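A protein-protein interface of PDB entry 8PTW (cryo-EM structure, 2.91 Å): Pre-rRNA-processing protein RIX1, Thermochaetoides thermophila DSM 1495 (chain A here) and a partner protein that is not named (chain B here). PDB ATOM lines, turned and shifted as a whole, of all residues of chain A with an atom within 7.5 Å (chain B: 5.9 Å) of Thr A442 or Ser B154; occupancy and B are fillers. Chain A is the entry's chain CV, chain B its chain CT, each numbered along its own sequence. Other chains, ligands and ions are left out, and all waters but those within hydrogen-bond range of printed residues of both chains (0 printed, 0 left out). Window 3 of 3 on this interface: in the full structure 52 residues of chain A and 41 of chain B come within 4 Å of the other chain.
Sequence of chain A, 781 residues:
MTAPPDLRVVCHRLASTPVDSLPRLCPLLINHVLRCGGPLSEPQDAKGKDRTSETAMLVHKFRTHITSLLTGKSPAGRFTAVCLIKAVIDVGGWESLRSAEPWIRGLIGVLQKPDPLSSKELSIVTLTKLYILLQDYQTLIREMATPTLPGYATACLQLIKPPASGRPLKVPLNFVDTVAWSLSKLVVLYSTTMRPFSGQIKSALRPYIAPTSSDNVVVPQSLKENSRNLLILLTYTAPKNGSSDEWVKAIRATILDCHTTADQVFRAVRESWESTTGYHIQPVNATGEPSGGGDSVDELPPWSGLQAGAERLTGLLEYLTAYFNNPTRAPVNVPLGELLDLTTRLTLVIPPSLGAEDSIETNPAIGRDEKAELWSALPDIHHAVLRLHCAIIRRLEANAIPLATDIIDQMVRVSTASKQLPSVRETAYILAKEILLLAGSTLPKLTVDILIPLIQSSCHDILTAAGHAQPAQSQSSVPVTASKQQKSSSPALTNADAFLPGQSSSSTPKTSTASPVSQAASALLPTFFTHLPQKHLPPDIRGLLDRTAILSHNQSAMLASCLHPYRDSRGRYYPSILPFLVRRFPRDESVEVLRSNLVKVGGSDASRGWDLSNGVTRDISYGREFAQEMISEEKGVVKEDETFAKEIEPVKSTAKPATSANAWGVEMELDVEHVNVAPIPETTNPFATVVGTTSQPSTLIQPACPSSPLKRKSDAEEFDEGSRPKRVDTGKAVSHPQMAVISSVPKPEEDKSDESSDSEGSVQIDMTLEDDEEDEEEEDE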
ATOM      1  N   ILE A 401      -3.475  10.172   5.558  1.00  0.00           N
ATOM      2  CA  ILE A 401      -2.647  10.853   4.554  1.00  0.00           C
ATOM      3  C   ILE A 401      -2.924  10.400   3.123  1.00  0.00           C
ATOM      4  O   ILE A 401      -2.994  11.266   2.237  1.00  0.00           O
ATOM      5  CB  ILE A 401      -1.165  10.765   4.951  1.00  0.00           C
ATOM      6  CG1 ILE A 401      -0.893  11.644   6.171  1.00  0.00           C
ATOM      7  CG2 ILE A 401      -0.241  11.170   3.808  1.00  0.00           C
ATOM      8  CD1 ILE A 401       0.526  11.558   6.683  1.00  0.00           C
ATOM      9  N   PRO A 402      -3.089   9.099   2.803  1.00  0.00           N
ATOM     10  CA  PRO A 402      -3.404   8.746   1.401  1.00  0.00           C
ATOM     11  C   PRO A 402      -4.712   9.313   0.864  1.00  0.00           C
ATOM     12  O   PRO A 402      -4.861   9.426  -0.359  1.00  0.00           O
ATOM     13  CB  PRO A 402      -3.439   7.215   1.428  1.00  0.00           C
ATOM     14  CG  PRO A 402      -2.531   6.848   2.495  1.00  0.00           C
ATOM     15  CD  PRO A 402      -2.715   7.881   3.555  1.00  0.00           C
ATOM     16  N   ALA A 404      -5.759  12.378   1.399  1.00  0.00           N
ATOM     17  CA  ALA A 404      -5.701  13.833   1.514  1.00  0.00           C
ATOM     18  C   ALA A 404      -6.005  14.525   0.193  1.00  0.00           C
ATOM     19  O   ALA A 404      -6.723  15.528   0.172  1.00  0.00           O
ATOM     20  CB  ALA A 404      -4.331  14.265   2.034  1.00  0.00           C
ATOM     21  N   THR A 405      -5.473  14.006  -0.918  1.00  0.00           N
ATOM     22  CA  THR A 405      -5.687  14.640  -2.217  1.00  0.00           C
ATOM     23  C   THR A 405      -7.157  14.601  -2.621  1.00  0.00           C
ATOM     24  O   THR A 405      -7.709  15.606  -3.094  1.00  0.00           O
ATOM     25  CB  THR A 405      -4.826  13.954  -3.278  1.00  0.00           C
ATOM     26  OG1 THR A 405      -3.460  13.938  -2.848  1.00  0.00           O
ATOM     27  CG2 THR A 405      -4.923  14.686  -4.608  1.00  0.00           C
ATOM     28  N   LEU A 436      -4.616  20.464   6.421  1.00  0.00           N
ATOM     29  CA  LEU A 436      -3.304  21.095   6.362  1.00  0.00           C
ATOM     30  C   LEU A 436      -2.422  20.632   7.514  1.00  0.00           C
ATOM     31  O   LEU A 436      -1.200  20.537   7.364  1.00  0.00           O
ATOM     32  CB  LEU A 436      -3.452  22.615   6.355  1.00  0.00           C
ATOM     33  CG  LEU A 436      -4.112  23.255   5.129  1.00  0.00           C
ATOM     34  CD1 LEU A 436      -3.850  24.750   5.107  1.00  0.00           C
ATOM     35  CD2 LEU A 436      -3.654  22.605   3.833  1.00  0.00           C
ATOM     36  N   LEU A 438      -2.430  17.592   8.634  1.00  0.00           N
ATOM     37  CA  LEU A 438      -1.885  16.300   8.227  1.00  0.00           C
ATOM     38  C   LEU A 438      -0.873  16.439   7.096  1.00  0.00           C
ATOM     39  O   LEU A 438       0.308  16.115   7.266  1.00  0.00           O
ATOM     40  CB  LEU A 438      -2.996  15.349   7.793  1.00  0.00           C
ATOM     41  CG  LEU A 438      -3.994  14.885   8.839  1.00  0.00           C
ATOM     42  CD1 LEU A 438      -5.060  14.065   8.145  1.00  0.00           C
ATOM     43  CD2 LEU A 438      -3.301  14.102   9.928  1.00  0.00           C
ATOM     44  N   ALA A 439      -1.315  16.917   5.933  1.00  0.00           N
ATOM     45  CA  ALA A 439      -0.499  16.874   4.730  1.00  0.00           C
ATOM     46  C   ALA A 439      -0.445  18.192   3.974  1.00  0.00           C
ATOM     47  O   ALA A 439      -0.350  18.172   2.742  1.00  0.00           O
ATOM     48  CB  ALA A 439      -1.004  15.776   3.784  1.00  0.00           C
ATOM     49  N   GLY A 440      -0.500  19.328   4.664  1.00  0.00           N
ATOM     50  CA  GLY A 440      -0.498  20.600   3.963  1.00  0.00           C
ATOM     51  C   GLY A 440       0.894  21.073   3.590  1.00  0.00           C
ATOM     52  O   GLY A 440       1.056  21.874   2.670  1.00  0.00           O
ATOM     53  N   SER A 441       1.915  20.578   4.293  1.00  0.00           N
ATOM     54  CA  SER A 441       3.258  21.131   4.141  1.00  0.00           C
ATOM     55  C   SER A 441       3.892  20.733   2.814  1.00  0.00           C
ATOM     56  O   SER A 441       4.707  21.478   2.259  1.00  0.00           O
ATOM     57  CB  SER A 441       4.141  20.685   5.305  1.00  0.00           C
ATOM     58  OG  SER A 441       3.516  20.952   6.546  1.00  0.00           O
ATOM     59  N   THR A 442       3.541  19.562   2.292  1.00  0.00           N
ATOM     60  CA  THR A 442       4.151  19.047   1.075  1.00  0.00           C
ATOM     61  C   THR A 442       3.236  19.129  -0.139  1.00  0.00           C
ATOM     62  O   THR A 442       3.393  18.327  -1.066  1.00  0.00           O
ATOM     63  CB  THR A 442       4.589  17.595   1.283  1.00  0.00           C
ATOM     64  OG1 THR A 442       3.466  16.817   1.716  1.00  0.00           O
ATOM     65  CG2 THR A 442       5.682  17.517   2.329  1.00  0.00           C
ATOM     66  N   LEU A 443       2.290  20.062  -0.156  1.00  0.00           N
ATOM     67  CA  LEU A 443       1.335  20.130  -1.252  1.00  0.00           C
ATOM     68  C   LEU A 443       2.009  20.656  -2.518  1.00  0.00           C
ATOM     69  O   LEU A 443       2.930  21.477  -2.438  1.00  0.00           O
ATOM     70  CB  LEU A 443       0.155  21.026  -0.875  1.00  0.00           C
ATOM     71  CG  LEU A 443      -0.828  20.436   0.136  1.00  0.00           C
ATOM     72  CD1 LEU A 443      -1.951  21.414   0.422  1.00  0.00           C
ATOM     73  CD2 LEU A 443      -1.381  19.117  -0.368  1.00  0.00           C
ATOM     74  N   PRO A 444       1.586  20.203  -3.697  1.00  0.00           N
ATOM     75  CA  PRO A 444       2.121  20.760  -4.943  1.00  0.00           C
ATOM     76  C   PRO A 444       1.527  22.131  -5.241  1.00  0.00           C
ATOM     77  O   PRO A 444       0.711  22.669  -4.492  1.00  0.00           O
ATOM     78  CB  PRO A 444       1.711  19.729  -5.996  1.00  0.00           C
ATOM     79  CG  PRO A 444       0.490  19.105  -5.437  1.00  0.00           C
ATOM     80  CD  PRO A 444       0.694  19.057  -3.948  1.00  0.00           C
ATOM     81  N   LYS A 445       1.963  22.696  -6.370  1.00  0.00           N
ATOM     82  CA  LYS A 445       1.551  24.047  -6.742  1.00  0.00           C
ATOM     83  C   LYS A 445       0.072  24.110  -7.102  1.00  0.00           C
ATOM     84  O   LYS A 445      -0.622  25.061  -6.723  1.00  0.00           O
ATOM     85  CB  LYS A 445       2.408  24.550  -7.907  1.00  0.00           C
ATOM     86  CG  LYS A 445       2.088  25.966  -8.375  1.00  0.00           C
ATOM     87  CD  LYS A 445       2.486  27.014  -7.352  1.00  0.00           C
ATOM     88  CE  LYS A 445       2.253  28.417  -7.891  1.00  0.00           C
ATOM     89  NZ  LYS A 445       2.570  29.478  -6.894  1.00  0.00           N
ATOM     90  N   THR A 447      -2.482  22.209  -6.148  1.00  0.00           N
ATOM     91  CA  THR A 447      -3.327  22.105  -4.964  1.00  0.00           C
ATOM     92  C   THR A 447      -3.401  23.427  -4.210  1.00  0.00           C
ATOM     93  O   THR A 447      -4.484  23.832  -3.772  1.00  0.00           O
ATOM     94  CB  THR A 447      -2.808  20.994  -4.054  1.00  0.00           C
ATOM     95  OG1 THR A 447      -2.738  19.768  -4.792  1.00  0.00           O
ATOM     96  CG2 THR A 447      -3.727  20.801  -2.871  1.00  0.00           C
ATOM     97  N   VAL A 448      -2.273  24.129  -4.079  1.00  0.00           N
ATOM     98  CA  VAL A 448      -2.281  25.453  -3.462  1.00  0.00           C
ATOM     99  C   VAL A 448      -3.115  26.422  -4.294  1.00  0.00           C
ATOM    100  O   VAL A 448      -3.881  27.230  -3.751  1.00  0.00           O
ATOM    101  CB  VAL A 448      -0.838  25.957  -3.265  1.00  0.00           C
ATOM    102  CG1 VAL A 448      -0.828  27.372  -2.722  1.00  0.00           C
ATOM    103  CG2 VAL A 448      -0.080  25.036  -2.326  1.00  0.00           C
ATOM    104  N   HIS A 531       1.276  25.501   8.151  1.00  0.00           N
ATOM    105  CA  HIS A 531       1.171  24.242   7.431  1.00  0.00           C
ATOM    106  C   HIS A 531       0.783  24.407   5.969  1.00  0.00           C
ATOM    107  O   HIS A 531       0.086  23.545   5.429  1.00  0.00           O
ATOM    108  CB  HIS A 531       0.167  23.332   8.136  1.00  0.00           C
ATOM    109  CG  HIS A 531       0.688  22.735   9.403  1.00  0.00           C
ATOM    110  ND1 HIS A 531       0.597  23.377  10.619  1.00  0.00           N
ATOM    111  CD2 HIS A 531       1.319  21.563   9.644  1.00  0.00           C
ATOM    112  CE1 HIS A 531       1.146  22.623  11.554  1.00  0.00           C
ATOM    113  NE2 HIS A 531       1.590  21.515  10.989  1.00  0.00           N
ATOM    114  N   LEU A 532       1.204  25.484   5.321  1.00  0.00           N
ATOM    115  CA  LEU A 532       0.999  25.663   3.896  1.00  0.00           C
ATOM    116  C   LEU A 532       2.294  26.136   3.263  1.00  0.00           C
ATOM    117  O   LEU A 532       3.033  26.900   3.900  1.00  0.00           O
ATOM    118  CB  LEU A 532      -0.118  26.680   3.640  1.00  0.00           C
ATOM    119  CG  LEU A 532      -0.854  26.655   2.301  1.00  0.00           C
ATOM    120  CD1 LEU A 532      -1.587  25.340   2.118  1.00  0.00           C
ATOM    121  CD2 LEU A 532      -1.823  27.816   2.219  1.00  0.00           C
ATOM    122  N   PRO A 533       2.627  25.699   2.042  1.00  0.00           N
ATOM    123  CA  PRO A 533       3.863  26.170   1.406  1.00  0.00           C
ATOM    124  C   PRO A 533       3.796  27.645   1.048  1.00  0.00           C
ATOM    125  O   PRO A 533       2.965  28.055   0.232  1.00  0.00           O
ATOM    126  CB  PRO A 533       3.969  25.292   0.153  1.00  0.00           C
ATOM    127  CG  PRO A 533       3.161  24.087   0.471  1.00  0.00           C
ATOM    128  CD  PRO A 533       2.012  24.607   1.274  1.00  0.00           C
ATOM    129  N   HIS A 536       4.504  28.651  -2.705  1.00  0.00           N
ATOM    130  CA  HIS A 536       3.466  28.468  -3.713  1.00  0.00           C
ATOM    131  C   HIS A 536       2.423  29.577  -3.651  1.00  0.00           C
ATOM    132  O   HIS A 536       1.679  29.790  -4.613  1.00  0.00           O
ATOM    133  CB  HIS A 536       2.809  27.100  -3.541  1.00  0.00           C
ATOM    134  CG  HIS A 536       3.723  25.955  -3.839  1.00  0.00           C
ATOM    135  ND1 HIS A 536       4.746  26.042  -4.758  1.00  0.00           N
ATOM    136  CD2 HIS A 536       3.768  24.695  -3.347  1.00  0.00           C
ATOM    137  CE1 HIS A 536       5.383  24.887  -4.816  1.00  0.00           C
ATOM    138  NE2 HIS A 536       4.809  24.052  -3.970  1.00  0.00           N
ATOM    139  N   SER B 137       6.112  14.440   7.675  1.00  0.00           N
ATOM    140  CA  SER B 137       5.910  14.989   6.339  1.00  0.00           C
ATOM    141  C   SER B 137       6.876  14.418   5.305  1.00  0.00           C
ATOM    142  O   SER B 137       6.487  14.229   4.148  1.00  0.00           O
ATOM    143  CB  SER B 137       6.033  16.512   6.377  1.00  0.00           C
ATOM    144  OG  SER B 137       7.261  16.907   6.962  1.00  0.00           O
ATOM    145  N   HIS B 138       8.122  14.143   5.684  1.00  0.00           N
ATOM    146  CA  HIS B 138       9.146  13.717   4.740  1.00  0.00           C
ATOM    147  C   HIS B 138       9.793  12.421   5.202  1.00  0.00           C
ATOM    148  O   HIS B 138       9.717  12.050   6.376  1.00  0.00           O
ATOM    149  CB  HIS B 138      10.238  14.784   4.566  1.00  0.00           C
ATOM    150  CG  HIS B 138       9.766  16.035   3.893  1.00  0.00           C
ATOM    151  ND1 HIS B 138       9.183  17.077   4.580  1.00  0.00           N
ATOM    152  CD2 HIS B 138       9.807  16.418   2.595  1.00  0.00           C
ATOM    153  CE1 HIS B 138       8.877  18.044   3.734  1.00  0.00           C
ATOM    154  NE2 HIS B 138       9.244  17.668   2.523  1.00  0.00           N
ATOM    155  N   SER B 152       8.714  13.019  -0.234  1.00  0.00           N
ATOM    156  CA  SER B 152       7.481  13.467   0.400  1.00  0.00           C
ATOM    157  C   SER B 152       6.631  12.256   0.753  1.00  0.00           C
ATOM    158  O   SER B 152       6.390  11.397  -0.100  1.00  0.00           O
ATOM    159  CB  SER B 152       6.698  14.402  -0.521  1.00  0.00           C
ATOM    160  OG  SER B 152       5.372  14.578  -0.060  1.00  0.00           O
ATOM    161  N   LEU B 153       6.185  12.187   2.010  1.00  0.00           N
ATOM    162  CA  LEU B 153       5.301  11.102   2.425  1.00  0.00           C
ATOM    163  C   LEU B 153       3.964  11.172   1.705  1.00  0.00           C
ATOM    164  O   LEU B 153       3.365  10.135   1.392  1.00  0.00           O
ATOM    165  CB  LEU B 153       5.079  11.147   3.934  1.00  0.00           C
ATOM    166  CG  LEU B 153       5.998  10.318   4.822  1.00  0.00           C
ATOM    167  CD1 LEU B 153       5.754  10.665   6.266  1.00  0.00           C
ATOM    168  CD2 LEU B 153       5.732   8.856   4.594  1.00  0.00           C
ATOM    169  N   SER B 154       3.480  12.386   1.438  1.00  0.00           N
ATOM    170  CA  SER B 154       2.163  12.553   0.835  1.00  0.00           C
ATOM    171  C   SER B 154       2.126  12.010  -0.587  1.00  0.00           C
ATOM    172  O   SER B 154       1.125  11.420  -1.003  1.00  0.00           O
ATOM    173  CB  SER B 154       1.764  14.027   0.859  1.00  0.00           C
ATOM    174  OG  SER B 154       1.635  14.489   2.191  1.00  0.00           O
ATOM    175  N   GLN B 155       3.209  12.189  -1.346  1.00  0.00           N
ATOM    176  CA  GLN B 155       3.230  11.693  -2.719  1.00  0.00           C
ATOM    177  C   GLN B 155       3.413  10.181  -2.766  1.00  0.00           C
ATOM    178  O   GLN B 155       2.869   9.513  -3.652  1.00  0.00           O
ATOM    179  CB  GLN B 155       4.329  12.390  -3.517  1.00  0.00           C
ATOM    180  CG  GLN B 155       4.166  13.895  -3.615  1.00  0.00           C
ATOM    181  CD  GLN B 155       5.238  14.542  -4.468  1.00  0.00           C
ATOM    182  OE1 GLN B 155       6.133  13.868  -4.978  1.00  0.00           O
ATOM    183  NE2 GLN B 155       5.152  15.857  -4.630  1.00  0.00           N
ATOM    184  N   LEU B 156       4.187   9.622  -1.833  1.00  0.00           N
ATOM    185  CA  LEU B 156       4.387   8.175  -1.812  1.00  0.00           C
ATOM    186  C   LEU B 156       3.128   7.446  -1.361  1.00  0.00           C
ATOM    187  O   LEU B 156       2.778   6.394  -1.906  1.00  0.00           O
ATOM    188  CB  LEU B 156       5.562   7.807  -0.902  1.00  0.00           C
ATOM    189  CG  LEU B 156       6.941   8.393  -1.197  1.00  0.00           C
ATOM    190  CD1 LEU B 156       7.861   8.220   0.001  1.00  0.00           C
ATOM    191  CD2 LEU B 156       7.543   7.753  -2.428  1.00  0.00           C
ATOM    192  N   LEU B 157       2.433   7.992  -0.362  1.00  0.00           N
ATOM    193  CA  LEU B 157       1.378   7.231   0.295  1.00  0.00           C
ATOM    194  C   LEU B 157       0.064   7.281  -0.473  1.00  0.00           C
ATOM    195  O   LEU B 157      -0.775   6.384  -0.325  1.00  0.00           O
ATOM    196  CB  LEU B 157       1.180   7.747   1.717  1.00  0.00           C
ATOM    197  CG  LEU B 157       2.251   7.356   2.730  1.00  0.00           C
ATOM    198  CD1 LEU B 157       1.969   8.026   4.057  1.00  0.00           C
ATOM    199  CD2 LEU B 157       2.289   5.850   2.884  1.00  0.00           C
ATOM    200  N   GLU B 158      -0.141   8.310  -1.293  1.00  0.00           N
ATOM    201  CA  GLU B 158      -1.481   8.579  -1.805  1.00  0.00           C
ATOM    202  C   GLU B 158      -1.879   7.573  -2.882  1.00  0.00           C
ATOM    203  O   GLU B 158      -1.031   6.953  -3.527  1.00  0.00           O
ATOM    204  CB  GLU B 158      -1.583  10.027  -2.297  1.00  0.00           C
ATOM    205  CG  GLU B 158      -0.690  10.455  -3.445  1.00  0.00           C
ATOM    206  CD  GLU B 158      -1.318  10.229  -4.789  1.00  0.00           C
ATOM    207  OE1 GLU B 158      -2.555  10.087  -4.841  1.00  0.00           O
ATOM    208  OE2 GLU B 158      -0.586  10.255  -5.795  1.00  0.00           O
ATOM    209  N   LEU B 168      11.810  14.504  -3.725  1.00  0.00           N
ATOM    210  CA  LEU B 168      11.774  15.958  -3.818  1.00  0.00           C
ATOM    211  C   LEU B 168      13.173  16.526  -3.986  1.00  0.00           C
ATOM    212  O   LEU B 168      13.397  17.399  -4.833  1.00  0.00           O
ATOM    213  CB  LEU B 168      11.110  16.570  -2.586  1.00  0.00           C
ATOM    214  CG  LEU B 168       9.780  16.024  -2.089  1.00  0.00           C
ATOM    215  CD1 LEU B 168       9.315  16.885  -0.933  1.00  0.00           C
ATOM    216  CD2 LEU B 168       8.758  16.018  -3.205  1.00  0.00           C
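Of chain B, only Ser B137, His B138, Ser B152 and Ser B154 come within 4 Å of Thr A442.
Printed residues of chain A within 4 Å of Ser B152: Thr A442 (3.4 Å).
Of the printed residues of chain A, His B138 touches Thr A442.
Of the printed residues of chain A, Ser B137 touches Thr A442 (3.8 Å).
Printed residues of chain B within 4 Å of Ala A439: Ser B154 (3.3 Å).
Of the printed residues of chain A, Glu B158 touches Pro A402 (3.7 Å).
Thr A405 touches none of the printed residues of chain B.
The nearest residue of chain A that does not touch Ser B154 is Ile A401 (4.1 Å).
Leu B157 touches Ile A401.
Leu B157 touches Pro A402 (O to CB, 3.3 Å).
CA of Glu B158 touches CA of Pro A402, at 3.7 Å.
CB of Ala A439 touches OG of Ser B154 (3.3 Å).
Ser B137 touches Thr A442 (O to CG2, 3.8 Å).
Thr A442 touches His B138 (CG2 to CE1, 3.5 Å).
The side-chain hydroxyl (OG) of Ser B137 lies within hydrogen-bond range of a ring nitrogen (ND1) of His B138 (3.1 Å).
O of Ser B137 sits at hydrogen-bond distance from N of Leu B153 (3.0 Å).
OG of Ser B152 lies close to N of Ser B154.
OG of Ser B152 lies within hydrogen-bond range of N of Gln B155, at 3.5 Å.
OG of Ser B152 sits close to OG1 of Thr A442 (3.4 Å).
The side-chain hydroxyl (OG1) of Thr A442 lies within hydrogen-bond range of the side-chain hydroxyl (OG) of Ser B154, 3.0 Å away.
Of the 10 printed residues of chain B, 6 touch a printed residue of chain A.
Along chain B the printed residues that touch a printed residue of chain A span positions 137 to 158.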
